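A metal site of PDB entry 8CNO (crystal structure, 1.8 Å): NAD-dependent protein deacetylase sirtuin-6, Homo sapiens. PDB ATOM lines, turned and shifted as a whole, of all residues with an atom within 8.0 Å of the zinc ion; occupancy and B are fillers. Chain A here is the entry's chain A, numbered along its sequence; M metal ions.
The side-chain sulfur (SG) of Cys 138 lies close to the side-chain hydroxyl (OG1) of Thr 140, 3.2 Å away.
SG of Cys 135 lies close to N of Lys 137.
The backbone carbonyl oxygen (O) of Thr 140 is in hydrogen-bond range of the backbone NH (N) of Cys 135 (3.0 Å).
The backbone NH (N) of Cys 160 lies within hydrogen-bond range of the backbone carbonyl oxygen (O) of Gly 173 (2.8 Å).
SG of Cys 160 sits close to N of Val 162 (3.8 Å).
O of Cys 160 sits at hydrogen-bond distance from N of Arg 172 (3.3 Å).
The side-chain sulfur (SG) of Cys 171 sits close to the backbone NH (N) of Gly 173 (3.6 Å).
The backbone carbonyl oxygen of Val 162 is in hydrogen-bond range of the backbone NH of Cys 171, at 3.4 Å.
The zinc ion is bound by SG of Cys 138 (2.3 Å), SG of Cys 135 (2.3 Å), SG of Cys 160 (2.3 Å) and SG of Cys 171 (2.4 Å).
The zinc ion has four donor atoms within binding distance.
Four residues have an atom within 4 Å of the zinc ion: Cys 135, Cys 138, Cys 160 and Cys 171.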
ATOM      1  N   GLU A 134       2.972   8.957  21.082  1.00  0.00           N
ATOM      2  CA  GLU A 134       2.703   7.671  21.783  1.00  0.00           C
ATOM      3  C   GLU A 134       3.470   6.537  21.101  1.00  0.00           C
ATOM      4  O   GLU A 134       3.416   6.405  19.839  1.00  0.00           O
ATOM      5  CB  GLU A 134       1.209   7.369  21.780  1.00  0.00           C
ATOM      6  CG  GLU A 134       0.859   6.049  22.445  1.00  0.00           C
ATOM      7  CD  GLU A 134      -0.638   5.871  22.553  1.00  0.00           C
ATOM      8  OE1 GLU A 134      -1.274   6.756  23.140  1.00  0.00           O
ATOM      9  OE2 GLU A 134      -1.171   4.883  22.028  1.00  0.00           O
ATOM     10  N   CYS A 135       4.122   5.710  21.911  1.00  0.00           N
ATOM     11  CA  CYS A 135       4.872   4.522  21.418  1.00  0.00           C
ATOM     12  C   CYS A 135       3.859   3.434  21.048  1.00  0.00           C
ATOM     13  O   CYS A 135       3.072   3.034  21.936  1.00  0.00           O
ATOM     14  CB  CYS A 135       5.824   3.998  22.475  1.00  0.00           C
ATOM     15  SG  CYS A 135       6.654   2.458  21.997  1.00  0.00           S
ATOM     16  N   ALA A 136       3.879   2.993  19.788  1.00  0.00           N
ATOM     17  CA  ALA A 136       2.991   1.916  19.310  1.00  0.00           C
ATOM     18  C   ALA A 136       3.219   0.631  20.129  1.00  0.00           C
ATOM     19  O   ALA A 136       2.216  -0.055  20.453  1.00  0.00           O
ATOM     20  CB  ALA A 136       3.212   1.686  17.847  1.00  0.00           C
ATOM     21  N   LYS A 137       4.472   0.339  20.500  1.00  0.00           N
ATOM     22  CA  LYS A 137       4.808  -0.908  21.230  1.00  0.00           C
ATOM     23  C   LYS A 137       4.295  -0.862  22.679  1.00  0.00           C
ATOM     24  O   LYS A 137       3.465  -1.739  22.999  1.00  0.00           O
ATOM     25  CB  LYS A 137       6.318  -1.185  21.170  1.00  0.00           C
ATOM     26  CG  LYS A 137       6.868  -1.414  19.769  1.00  0.00           C
ATOM     27  CD  LYS A 137       6.397  -2.705  19.146  1.00  0.00           C
ATOM     28  CE  LYS A 137       7.107  -3.040  17.855  1.00  0.00           C
ATOM     29  NZ  LYS A 137       6.541  -4.264  17.236  1.00  0.00           N
ATOM     30  N   CYS A 138       4.714   0.096  23.508  1.00  0.00           N
ATOM     31  CA  CYS A 138       4.414   0.055  24.964  1.00  0.00           C
ATOM     32  C   CYS A 138       3.393   1.114  25.409  1.00  0.00           C
ATOM     33  O   CYS A 138       3.077   1.110  26.605  1.00  0.00           O
ATOM     34  CB  CYS A 138       5.681   0.200  25.815  1.00  0.00           C
ATOM     35  SG  CYS A 138       6.392   1.865  25.769  1.00  0.00           S
ATOM     36  N   LYS A 139       2.929   1.988  24.516  1.00  0.00           N
ATOM     37  CA  LYS A 139       1.849   2.978  24.793  1.00  0.00           C
ATOM     38  C   LYS A 139       2.361   4.074  25.736  1.00  0.00           C
ATOM     39  O   LYS A 139       1.533   4.867  26.215  1.00  0.00           O
ATOM     40  CB  LYS A 139       0.596   2.291  25.341  1.00  0.00           C
ATOM     41  CG  LYS A 139       0.093   1.098  24.529  1.00  0.00           C
ATOM     42  CD  LYS A 139      -0.155   1.417  23.063  1.00  0.00           C
ATOM     43  CE  LYS A 139      -0.619   0.205  22.277  1.00  0.00           C
ATOM     44  NZ  LYS A 139      -0.554   0.432  20.827  1.00  0.00           N
ATOM     45  N   THR A 140       3.683   4.158  25.970  1.00  0.00           N
ATOM     46  CA  THR A 140       4.255   5.261  26.793  1.00  0.00           C
ATOM     47  C   THR A 140       4.040   6.544  25.992  1.00  0.00           C
ATOM     48  O   THR A 140       4.399   6.558  24.806  1.00  0.00           O
ATOM     49  CB  THR A 140       5.717   5.031  27.194  1.00  0.00           C
ATOM     50  OG1 THR A 140       5.738   3.931  28.092  1.00  0.00           O
ATOM     51  CG2 THR A 140       6.356   6.221  27.895  1.00  0.00           C
ATOM     52  N   GLN A 141       3.401   7.537  26.624  1.00  0.00           N
ATOM     53  CA  GLN A 141       3.185   8.889  26.051  1.00  0.00           C
ATOM     54  C   GLN A 141       4.331   9.818  26.435  1.00  0.00           C
ATOM     55  O   GLN A 141       4.952   9.639  27.481  1.00  0.00           O
ATOM     56  CB  GLN A 141       1.823   9.434  26.480  1.00  0.00           C
ATOM     57  CG  GLN A 141       0.693   8.609  25.886  1.00  0.00           C
ATOM     58  CD  GLN A 141      -0.685   9.165  26.107  1.00  0.00           C
ATOM     59  OE1 GLN A 141      -0.989   9.758  27.145  1.00  0.00           O
ATOM     60  NE2 GLN A 141      -1.545   8.986  25.114  1.00  0.00           N
ATOM     61  N   TYR A 142       4.654  10.722  25.522  1.00  0.00           N
ATOM     62  CA  TYR A 142       5.706  11.740  25.639  1.00  0.00           C
ATOM     63  C   TYR A 142       5.011  13.077  25.412  1.00  0.00           C
ATOM     64  O   TYR A 142       4.330  13.229  24.339  1.00  0.00           O
ATOM     65  CB  TYR A 142       6.824  11.473  24.624  1.00  0.00           C
ATOM     66  CG  TYR A 142       7.569  10.184  24.844  1.00  0.00           C
ATOM     67  CD1 TYR A 142       7.090   8.968  24.362  1.00  0.00           C
ATOM     68  CD2 TYR A 142       8.761  10.182  25.547  1.00  0.00           C
ATOM     69  CE1 TYR A 142       7.791   7.794  24.580  1.00  0.00           C
ATOM     70  CE2 TYR A 142       9.472   9.026  25.754  1.00  0.00           C
ATOM     71  CZ  TYR A 142       8.978   7.815  25.299  1.00  0.00           C
ATOM     72  OH  TYR A 142       9.722   6.682  25.519  1.00  0.00           O
ATOM     73  N   LEU A 159      11.951   7.461  18.395  1.00  0.00           N
ATOM     74  CA  LEU A 159      11.847   6.114  19.013  1.00  0.00           C
ATOM     75  C   LEU A 159      11.703   6.244  20.528  1.00  0.00           C
ATOM     76  O   LEU A 159      12.262   7.190  21.134  1.00  0.00           O
ATOM     77  CB  LEU A 159      13.078   5.275  18.634  1.00  0.00           C
ATOM     78  CG  LEU A 159      13.301   5.084  17.141  1.00  0.00           C
ATOM     79  CD1 LEU A 159      14.506   4.188  16.888  1.00  0.00           C
ATOM     80  CD2 LEU A 159      12.073   4.516  16.449  1.00  0.00           C
ATOM     81  N   CYS A 160      10.955   5.312  21.089  1.00  0.00           N
ATOM     82  CA  CYS A 160      10.720   5.139  22.528  1.00  0.00           C
ATOM     83  C   CYS A 160      12.062   5.005  23.248  1.00  0.00           C
ATOM     84  O   CYS A 160      12.919   4.272  22.702  1.00  0.00           O
ATOM     85  CB  CYS A 160       9.889   3.892  22.753  1.00  0.00           C
ATOM     86  SG  CYS A 160       9.122   3.893  24.376  1.00  0.00           S
ATOM     87  N   THR A 161      12.230   5.658  24.389  1.00  0.00           N
ATOM     88  CA  THR A 161      13.490   5.625  25.206  1.00  0.00           C
ATOM     89  C   THR A 161      13.264   4.848  26.503  1.00  0.00           C
ATOM     90  O   THR A 161      14.140   4.901  27.382  1.00  0.00           O
ATOM     91  CB  THR A 161      14.006   7.044  25.479  1.00  0.00           C
ATOM     92  OG1 THR A 161      12.994   7.758  26.200  1.00  0.00           O
ATOM     93  CG2 THR A 161      14.374   7.786  24.208  1.00  0.00           C
ATOM     94  N   VAL A 162      12.140   4.150  26.648  1.00  0.00           N
ATOM     95  CA  VAL A 162      11.793   3.412  27.905  1.00  0.00           C
ATOM     96  C   VAL A 162      12.843   2.303  28.135  1.00  0.00           C
ATOM     97  O   VAL A 162      13.121   1.555  27.163  1.00  0.00           O
ATOM     98  CB  VAL A 162      10.357   2.872  27.835  1.00  0.00           C
ATOM     99  CG1 VAL A 162      10.062   1.849  28.917  1.00  0.00           C
ATOM    100  CG2 VAL A 162       9.357   4.011  27.892  1.00  0.00           C
ATOM    101  N   ALA A 163      13.375   2.202  29.360  1.00  0.00           N
ATOM    102  CA  ALA A 163      14.539   1.353  29.734  1.00  0.00           C
ATOM    103  C   ALA A 163      14.530   0.051  28.924  1.00  0.00           C
ATOM    104  O   ALA A 163      13.574  -0.720  29.118  1.00  0.00           O
ATOM    105  CB  ALA A 163      14.536   1.070  31.218  1.00  0.00           C
ATOM    106  N   CYS A 171      13.145  -0.279  24.333  1.00  0.00           N
ATOM    107  CA  CYS A 171      11.892  -0.443  23.552  1.00  0.00           C
ATOM    108  C   CYS A 171      12.137  -0.099  22.081  1.00  0.00           C
ATOM    109  O   CYS A 171      11.785  -0.930  21.226  1.00  0.00           O
ATOM    110  CB  CYS A 171      10.789   0.440  24.129  1.00  0.00           C
ATOM    111  SG  CYS A 171       9.200   0.194  23.287  1.00  0.00           S
ATOM    112  N   ARG A 172      12.683   1.084  21.796  1.00  0.00           N
ATOM    113  CA  ARG A 172      12.964   1.592  20.425  1.00  0.00           C
ATOM    114  C   ARG A 172      11.701   1.497  19.566  1.00  0.00           C
ATOM    115  O   ARG A 172      11.811   1.521  18.324  1.00  0.00           O
ATOM    116  CB  ARG A 172      14.153   0.839  19.809  1.00  0.00           C
ATOM    117  CG  ARG A 172      15.467   1.067  20.551  1.00  0.00           C
ATOM    118  CD  ARG A 172      16.645   0.358  19.931  1.00  0.00           C
ATOM    119  NE  ARG A 172      16.574   0.361  18.468  1.00  0.00           N
ATOM    120  CZ  ARG A 172      16.952   1.364  17.679  1.00  0.00           C
ATOM    121  NH1 ARG A 172      17.461   2.470  18.189  1.00  0.00           N
ATOM    122  NH2 ARG A 172      16.814   1.250  16.367  1.00  0.00           N
ATOM    123  N   GLY A 173      10.528   1.533  20.208  1.00  0.00           N
ATOM    124  CA  GLY A 173       9.225   1.503  19.521  1.00  0.00           C
ATOM    125  C   GLY A 173       8.962   2.791  18.763  1.00  0.00           C
ATOM    126  O   GLY A 173       9.403   3.863  19.255  1.00  0.00           O
ATOM    127  N   GLU A 174       8.336   2.672  17.594  1.00  0.00           N
ATOM    128  CA  GLU A 174       7.849   3.783  16.730  1.00  0.00           C
ATOM    129  C   GLU A 174       6.929   4.698  17.550  1.00  0.00           C
ATOM    130  O   GLU A 174       5.890   4.228  18.016  1.00  0.00           O
ATOM    131  CB  GLU A 174       7.110   3.183  15.534  1.00  0.00           C
ATOM    132  CG  GLU A 174       6.740   4.195  14.454  1.00  0.00           C
ATOM    133  CD  GLU A 174       6.266   3.569  13.141  1.00  0.00           C
ATOM    134  OE1 GLU A 174       7.132   3.086  12.372  1.00  0.00           O
ATOM    135  OE2 GLU A 174       5.042   3.572  12.895  1.00  0.00           O
ATOM    136  N   LEU A 175       7.334   5.962  17.714  1.00  0.00           N
ATOM    137  CA  LEU A 175       6.442   7.052  18.211  1.00  0.00           C
ATOM    138  C   LEU A 175       5.490   7.511  17.110  1.00  0.00           C
ATOM    139  O   LEU A 175       5.893   7.658  15.918  1.00  0.00           O
ATOM    140  CB  LEU A 175       7.302   8.185  18.777  1.00  0.00           C
ATOM    141  CG  LEU A 175       8.192   7.737  19.947  1.00  0.00           C
ATOM    142  CD1 LEU A 175       8.808   8.914  20.662  1.00  0.00           C
ATOM    143  CD2 LEU A 175       7.403   6.865  20.901  1.00  0.00           C
HETATM  144 ZN    ZN M   1       7.796   2.013  23.962  1.00  0.00          ZN
